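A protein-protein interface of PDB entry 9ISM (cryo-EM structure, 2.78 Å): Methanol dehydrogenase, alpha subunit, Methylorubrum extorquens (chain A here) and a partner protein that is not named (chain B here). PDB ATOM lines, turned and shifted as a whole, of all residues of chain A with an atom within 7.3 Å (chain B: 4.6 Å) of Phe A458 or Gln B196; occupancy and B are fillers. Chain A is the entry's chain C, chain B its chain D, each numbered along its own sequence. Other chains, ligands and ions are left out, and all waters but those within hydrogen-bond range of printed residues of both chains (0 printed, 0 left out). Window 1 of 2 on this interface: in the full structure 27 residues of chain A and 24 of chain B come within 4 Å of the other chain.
O of Ala A461 lies close to OD1 of Asn B195, at 3.0 Å. The backbone carbonyl oxygen (O) of Thr A580 sits at hydrogen-bond distance from the side-chain amide nitrogen (ND2) of Asn B195.
O of Gly A460 sits at hydrogen-bond distance from N of Phe A448, 2.9 Å away. O of Phe A458 is in hydrogen-bond range of N of Leu A450 (2.9 Å).
Among the printed residues, pairs that only touch across the chains: Phe A448 with Asn B195 (3.8 Å), Leu A450 with Ile B97 (3.95 Å), Pro A451 with Ile B97 (3.6 Å), Tyr A452 with Ile B97 (3.9 Å), Phe A458 with Arg B194 (3.3 Å), Phe A458 with Gln B196 (3.1 Å), Gly A460 with Arg B194 (3.8 Å) and Ala A461 with Arg B194 (3.9 Å).
Of the printed residues of chain B, Phe A458 touches Arg B194 and Gln B196. Gln B196 touches one residue of chain A. Printed residues of chain A within 4 Å of Asn B195: Phe A448 (3.8 Å), Ala A461 (3.0 Å) and Thr A580 (3.3 Å). Printed residues of chain B within 4 Å of Pro A451: Ile B97. Printed residues of chain A within 4 Å of Ile B97: Leu A450 (3.95 Å), Pro A451 (3.6 Å) and Tyr A452 (3.9 Å). Gln A456 touches none of the printed residues of chain B. The nearest residue of chain A that does not touch Gln B196 is Phe A448 (5.8 Å).
Hydrophobic or aromatic side chains of chain A that line the printed part of chain B: Phe A448, Tyr A452 and Phe A458. Along chain A the printed residues that touch a printed residue of chain B span positions 448 to 580. Printed residues of chain B that touch a printed residue of chain A: Ile B97, Arg B194, Asn B195 and Gln B196. Among the printed residues, no Asp or Glu carboxylate lies within 4 Å of a Lys or Arg side-chain nitrogen of the other chain.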
ATOM      1  N   TRP A 292     -20.455 -29.430 -21.332  1.00  0.00           N
ATOM      2  CA  TRP A 292     -19.775 -30.362 -20.439  1.00  0.00           C
ATOM      3  C   TRP A 292     -18.991 -29.665 -19.338  1.00  0.00           C
ATOM      4  O   TRP A 292     -18.663 -30.302 -18.333  1.00  0.00           O
ATOM      5  CB  TRP A 292     -18.843 -31.274 -21.238  1.00  0.00           C
ATOM      6  CG  TRP A 292     -17.627 -30.590 -21.783  1.00  0.00           C
ATOM      7  CD1 TRP A 292     -17.496 -30.008 -23.008  1.00  0.00           C
ATOM      8  CD2 TRP A 292     -16.365 -30.429 -21.126  1.00  0.00           C
ATOM      9  NE1 TRP A 292     -16.235 -29.489 -23.152  1.00  0.00           N
ATOM     10  CE2 TRP A 292     -15.521 -29.735 -22.010  1.00  0.00           C
ATOM     11  CE3 TRP A 292     -15.869 -30.802 -19.874  1.00  0.00           C
ATOM     12  CZ2 TRP A 292     -14.212 -29.405 -21.683  1.00  0.00           C
ATOM     13  CZ3 TRP A 292     -14.571 -30.474 -19.552  1.00  0.00           C
ATOM     14  CH2 TRP A 292     -13.756 -29.782 -20.452  1.00  0.00           C
ATOM     15  N   PHE A 448      -6.505 -29.329 -18.312  1.00  0.00           N
ATOM     16  CA  PHE A 448      -5.354 -28.606 -18.828  1.00  0.00           C
ATOM     17  C   PHE A 448      -5.821 -27.364 -19.574  1.00  0.00           C
ATOM     18  O   PHE A 448      -6.922 -27.330 -20.136  1.00  0.00           O
ATOM     19  CB  PHE A 448      -4.494 -29.490 -19.738  1.00  0.00           C
ATOM     20  CG  PHE A 448      -5.157 -29.872 -21.028  1.00  0.00           C
ATOM     21  CD1 PHE A 448      -6.018 -30.949 -21.085  1.00  0.00           C
ATOM     22  CD2 PHE A 448      -4.904 -29.167 -22.188  1.00  0.00           C
ATOM     23  CE1 PHE A 448      -6.622 -31.305 -22.270  1.00  0.00           C
ATOM     24  CE2 PHE A 448      -5.509 -29.520 -23.373  1.00  0.00           C
ATOM     25  CZ  PHE A 448      -6.366 -30.591 -23.413  1.00  0.00           C
ATOM     26  N   MET A 449      -4.964 -26.345 -19.559  1.00  0.00           N
ATOM     27  CA  MET A 449      -5.176 -25.104 -20.291  1.00  0.00           C
ATOM     28  C   MET A 449      -3.931 -24.797 -21.105  1.00  0.00           C
ATOM     29  O   MET A 449      -2.814 -24.856 -20.583  1.00  0.00           O
ATOM     30  CB  MET A 449      -5.488 -23.943 -19.345  1.00  0.00           C
ATOM     31  CG  MET A 449      -5.485 -22.586 -20.021  1.00  0.00           C
ATOM     32  SD  MET A 449      -6.032 -21.257 -18.939  1.00  0.00           S
ATOM     33  CE  MET A 449      -5.301 -19.842 -19.755  1.00  0.00           C
ATOM     34  N   LEU A 450      -4.123 -24.470 -22.379  1.00  0.00           N
ATOM     35  CA  LEU A 450      -3.024 -24.184 -23.293  1.00  0.00           C
ATOM     36  C   LEU A 450      -3.214 -22.803 -23.905  1.00  0.00           C
ATOM     37  O   LEU A 450      -4.224 -22.573 -24.591  1.00  0.00           O
ATOM     38  CB  LEU A 450      -2.941 -25.243 -24.391  1.00  0.00           C
ATOM     39  CG  LEU A 450      -2.149 -26.506 -24.065  1.00  0.00           C
ATOM     40  CD1 LEU A 450      -2.451 -27.591 -25.081  1.00  0.00           C
ATOM     41  CD2 LEU A 450      -0.663 -26.209 -24.023  1.00  0.00           C
ATOM     42  N   PRO A 451      -2.303 -21.862 -23.683  1.00  0.00           N
ATOM     43  CA  PRO A 451      -2.415 -20.549 -24.322  1.00  0.00           C
ATOM     44  C   PRO A 451      -1.950 -20.593 -25.773  1.00  0.00           C
ATOM     45  O   PRO A 451      -1.420 -21.591 -26.259  1.00  0.00           O
ATOM     46  CB  PRO A 451      -1.501 -19.663 -23.473  1.00  0.00           C
ATOM     47  CG  PRO A 451      -0.523 -20.595 -22.879  1.00  0.00           C
ATOM     48  CD  PRO A 451      -1.226 -21.902 -22.683  1.00  0.00           C
ATOM     49  N   TYR A 452      -2.162 -19.478 -26.459  1.00  0.00           N
ATOM     50  CA  TYR A 452      -1.826 -19.362 -27.874  1.00  0.00           C
ATOM     51  C   TYR A 452      -1.439 -17.911 -28.157  1.00  0.00           C
ATOM     52  O   TYR A 452      -1.151 -17.141 -27.235  1.00  0.00           O
ATOM     53  CB  TYR A 452      -2.991 -19.870 -28.741  1.00  0.00           C
ATOM     54  CG  TYR A 452      -2.629 -20.088 -30.191  1.00  0.00           C
ATOM     55  CD1 TYR A 452      -1.380 -20.563 -30.552  1.00  0.00           C
ATOM     56  CD2 TYR A 452      -3.534 -19.801 -31.198  1.00  0.00           C
ATOM     57  CE1 TYR A 452      -1.048 -20.754 -31.875  1.00  0.00           C
ATOM     58  CE2 TYR A 452      -3.210 -19.990 -32.523  1.00  0.00           C
ATOM     59  CZ  TYR A 452      -1.967 -20.465 -32.855  1.00  0.00           C
ATOM     60  OH  TYR A 452      -1.643 -20.654 -34.177  1.00  0.00           O
ATOM     61  N   GLN A 456      -5.820 -15.965 -26.854  1.00  0.00           N
ATOM     62  CA  GLN A 456      -6.576 -17.195 -27.008  1.00  0.00           C
ATOM     63  C   GLN A 456      -6.067 -18.245 -26.036  1.00  0.00           C
ATOM     64  O   GLN A 456      -4.899 -18.236 -25.639  1.00  0.00           O
ATOM     65  CB  GLN A 456      -6.485 -17.744 -28.430  1.00  0.00           C
ATOM     66  CG  GLN A 456      -6.857 -16.763 -29.513  1.00  0.00           C
ATOM     67  CD  GLN A 456      -6.804 -17.393 -30.885  1.00  0.00           C
ATOM     68  OE1 GLN A 456      -6.999 -18.598 -31.032  1.00  0.00           O
ATOM     69  NE2 GLN A 456      -6.535 -16.582 -31.900  1.00  0.00           N
ATOM     70  N   PHE A 457      -6.960 -19.151 -25.653  1.00  0.00           N
ATOM     71  CA  PHE A 457      -6.584 -20.280 -24.820  1.00  0.00           C
ATOM     72  C   PHE A 457      -7.591 -21.400 -25.026  1.00  0.00           C
ATOM     73  O   PHE A 457      -8.756 -21.163 -25.354  1.00  0.00           O
ATOM     74  CB  PHE A 457      -6.480 -19.873 -23.345  1.00  0.00           C
ATOM     75  CG  PHE A 457      -7.774 -19.411 -22.743  1.00  0.00           C
ATOM     76  CD1 PHE A 457      -8.133 -18.076 -22.795  1.00  0.00           C
ATOM     77  CD2 PHE A 457      -8.622 -20.302 -22.111  1.00  0.00           C
ATOM     78  CE1 PHE A 457      -9.319 -17.641 -22.239  1.00  0.00           C
ATOM     79  CE2 PHE A 457      -9.812 -19.872 -21.554  1.00  0.00           C
ATOM     80  CZ  PHE A 457     -10.159 -18.540 -21.618  1.00  0.00           C
ATOM     81  N   PHE A 458      -7.119 -22.628 -24.832  1.00  0.00           N
ATOM     82  CA  PHE A 458      -7.939 -23.825 -24.955  1.00  0.00           C
ATOM     83  C   PHE A 458      -7.981 -24.548 -23.617  1.00  0.00           C
ATOM     84  O   PHE A 458      -6.936 -24.795 -23.009  1.00  0.00           O
ATOM     85  CB  PHE A 458      -7.394 -24.754 -26.037  1.00  0.00           C
ATOM     86  CG  PHE A 458      -8.158 -26.032 -26.174  1.00  0.00           C
ATOM     87  CD1 PHE A 458      -9.484 -26.022 -26.560  1.00  0.00           C
ATOM     88  CD2 PHE A 458      -7.550 -27.246 -25.917  1.00  0.00           C
ATOM     89  CE1 PHE A 458     -10.192 -27.199 -26.686  1.00  0.00           C
ATOM     90  CE2 PHE A 458      -8.251 -28.425 -26.042  1.00  0.00           C
ATOM     91  CZ  PHE A 458      -9.573 -28.402 -26.427  1.00  0.00           C
ATOM     92  N   VAL A 459      -9.186 -24.890 -23.168  1.00  0.00           N
ATOM     93  CA  VAL A 459      -9.404 -25.583 -21.905  1.00  0.00           C
ATOM     94  C   VAL A 459      -9.979 -26.958 -22.209  1.00  0.00           C
ATOM     95  O   VAL A 459     -10.969 -27.069 -22.940  1.00  0.00           O
ATOM     96  CB  VAL A 459     -10.348 -24.795 -20.980  1.00  0.00           C
ATOM     97  CG1 VAL A 459     -10.434 -25.460 -19.621  1.00  0.00           C
ATOM     98  CG2 VAL A 459      -9.877 -23.364 -20.844  1.00  0.00           C
ATOM     99  N   GLY A 460      -9.364 -28.000 -21.652  1.00  0.00           N
ATOM    100  CA  GLY A 460      -9.818 -29.348 -21.919  1.00  0.00           C
ATOM    101  C   GLY A 460      -9.495 -30.280 -20.772  1.00  0.00           C
ATOM    102  O   GLY A 460      -8.942 -29.874 -19.750  1.00  0.00           O
ATOM    103  N   ALA A 461      -9.844 -31.551 -20.958  1.00  0.00           N
ATOM    104  CA  ALA A 461      -9.596 -32.582 -19.964  1.00  0.00           C
ATOM    105  C   ALA A 461      -9.219 -33.880 -20.659  1.00  0.00           C
ATOM    106  O   ALA A 461      -9.776 -34.213 -21.707  1.00  0.00           O
ATOM    107  CB  ALA A 461     -10.819 -32.804 -19.070  1.00  0.00           C
ATOM    108  N   THR A 580      -5.964 -42.070 -25.975  1.00  0.00           N
ATOM    109  CA  THR A 580      -6.819 -40.957 -25.578  1.00  0.00           C
ATOM    110  C   THR A 580      -8.028 -40.815 -26.496  1.00  0.00           C
ATOM    111  O   THR A 580      -9.055 -40.263 -26.086  1.00  0.00           O
ATOM    112  CB  THR A 580      -6.009 -39.660 -25.559  1.00  0.00           C
ATOM    113  OG1 THR A 580      -4.751 -39.895 -24.916  1.00  0.00           O
ATOM    114  CG2 THR A 580      -6.753 -38.570 -24.799  1.00  0.00           C
ATOM    115  N   ALA A 581      -7.932 -41.308 -27.729  1.00  0.00           N
ATOM    116  CA  ALA A 581      -9.038 -41.196 -28.668  1.00  0.00           C
ATOM    117  C   ALA A 581     -10.244 -41.988 -28.177  1.00  0.00           C
ATOM    118  O   ALA A 581     -10.112 -43.057 -27.576  1.00  0.00           O
ATOM    119  CB  ALA A 581      -8.615 -41.686 -30.052  1.00  0.00           C
ATOM    120  N   ILE B  97      -0.686 -24.636 -32.023  1.00  0.00           N
ATOM    121  CA  ILE B  97      -0.797 -24.427 -30.582  1.00  0.00           C
ATOM    122  C   ILE B  97       0.123 -25.370 -29.819  1.00  0.00           C
ATOM    123  O   ILE B  97       0.566 -25.053 -28.709  1.00  0.00           O
ATOM    124  CB  ILE B  97      -2.265 -24.573 -30.140  1.00  0.00           C
ATOM    125  CG1 ILE B  97      -2.441 -24.108 -28.695  1.00  0.00           C
ATOM    126  CG2 ILE B  97      -2.743 -26.004 -30.313  1.00  0.00           C
ATOM    127  CD1 ILE B  97      -3.881 -23.916 -28.291  1.00  0.00           C
ATOM    128  N   PRO B 193     -14.241 -32.575 -29.588  1.00  0.00           N
ATOM    129  CA  PRO B 193     -13.858 -33.348 -28.405  1.00  0.00           C
ATOM    130  C   PRO B 193     -13.030 -32.516 -27.440  1.00  0.00           C
ATOM    131  O   PRO B 193     -12.377 -31.538 -27.813  1.00  0.00           O
ATOM    132  CB  PRO B 193     -13.036 -34.507 -28.982  1.00  0.00           C
ATOM    133  CG  PRO B 193     -13.314 -34.499 -30.456  1.00  0.00           C
ATOM    134  CD  PRO B 193     -13.578 -33.075 -30.801  1.00  0.00           C
ATOM    135  N   ARG B 194     -13.070 -32.922 -26.172  1.00  0.00           N
ATOM    136  CA  ARG B 194     -12.303 -32.223 -25.147  1.00  0.00           C
ATOM    137  C   ARG B 194     -10.802 -32.373 -25.365  1.00  0.00           C
ATOM    138  O   ARG B 194     -10.041 -31.425 -25.147  1.00  0.00           O
ATOM    139  CB  ARG B 194     -12.691 -32.735 -23.763  1.00  0.00           C
ATOM    140  CG  ARG B 194     -14.095 -33.277 -23.683  1.00  0.00           C
ATOM    141  CD  ARG B 194     -14.321 -34.002 -22.377  1.00  0.00           C
ATOM    142  NE  ARG B 194     -15.557 -34.772 -22.399  1.00  0.00           N
ATOM    143  CZ  ARG B 194     -16.162 -35.246 -21.320  1.00  0.00           C
ATOM    144  NH1 ARG B 194     -15.671 -35.045 -20.108  1.00  0.00           N
ATOM    145  NH2 ARG B 194     -17.286 -35.939 -21.460  1.00  0.00           N
ATOM    146  N   ASN B 195     -10.358 -33.558 -25.788  1.00  0.00           N
ATOM    147  CA  ASN B 195      -8.926 -33.827 -25.871  1.00  0.00           C
ATOM    148  C   ASN B 195      -8.247 -32.969 -26.933  1.00  0.00           C
ATOM    149  O   ASN B 195      -7.180 -32.398 -26.684  1.00  0.00           O
ATOM    150  CB  ASN B 195      -8.688 -35.308 -26.158  1.00  0.00           C
ATOM    151  CG  ASN B 195      -9.451 -36.213 -25.215  1.00  0.00           C
ATOM    152  OD1 ASN B 195      -9.385 -36.056 -23.996  1.00  0.00           O
ATOM    153  ND2 ASN B 195     -10.182 -37.168 -25.776  1.00  0.00           N
ATOM    154  N   GLN B 196      -8.843 -32.862 -28.114  1.00  0.00           N
ATOM    155  CA  GLN B 196      -8.207 -32.202 -29.243  1.00  0.00           C
ATOM    156  C   GLN B 196      -8.703 -30.768 -29.392  1.00  0.00           C
ATOM    157  O   GLN B 196      -9.722 -30.366 -28.828  1.00  0.00           O
ATOM    158  CB  GLN B 196      -8.453 -32.992 -30.531  1.00  0.00           C
ATOM    159  CG  GLN B 196      -9.906 -33.347 -30.774  1.00  0.00           C
ATOM    160  CD  GLN B 196     -10.099 -34.198 -32.014  1.00  0.00           C
ATOM    161  OE1 GLN B 196      -9.581 -35.311 -32.104  1.00  0.00           O
ATOM    162  NE2 GLN B 196     -10.850 -33.678 -32.977  1.00  0.00           N
ATOM    163  N   TYR B 197      -7.958 -29.996 -30.178  1.00  0.00           N
ATOM    164  CA  TYR B 197      -8.198 -28.573 -30.371  1.00  0.00           C
ATOM    165  C   TYR B 197      -8.798 -28.340 -31.749  1.00  0.00           C
ATOM    166  O   TYR B 197      -8.226 -28.766 -32.759  1.00  0.00           O
ATOM    167  CB  TYR B 197      -6.891 -27.792 -30.207  1.00  0.00           C
ATOM    168  CG  TYR B 197      -6.866 -26.425 -30.846  1.00  0.00           C
ATOM    169  CD1 TYR B 197      -7.517 -25.351 -30.260  1.00  0.00           C
ATOM    170  CD2 TYR B 197      -6.173 -26.205 -32.024  1.00  0.00           C
ATOM    171  CE1 TYR B 197      -7.485 -24.098 -30.837  1.00  0.00           C
ATOM    172  CE2 TYR B 197      -6.136 -24.958 -32.608  1.00  0.00           C
ATOM    173  CZ  TYR B 197      -6.794 -23.908 -32.011  1.00  0.00           C
ATOM    174  OH  TYR B 197      -6.760 -22.663 -32.593  1.00  0.00           O
ATOM    175  N   THR B 198      -9.946 -27.666 -31.789  1.00  0.00           N
ATOM    176  CA  THR B 198     -10.670 -27.405 -33.025  1.00  0.00           C
ATOM    177  C   THR B 198     -10.873 -25.907 -33.203  1.00  0.00           C
ATOM    178  O   THR B 198     -11.128 -25.186 -32.233  1.00  0.00           O
ATOM    179  CB  THR B 198     -12.027 -28.110 -33.031  1.00  0.00           C
ATOM    180  OG1 THR B 198     -12.827 -27.617 -31.950  1.00  0.00           O
ATOM    181  CG2 THR B 198     -11.847 -29.611 -32.876  1.00  0.00           C
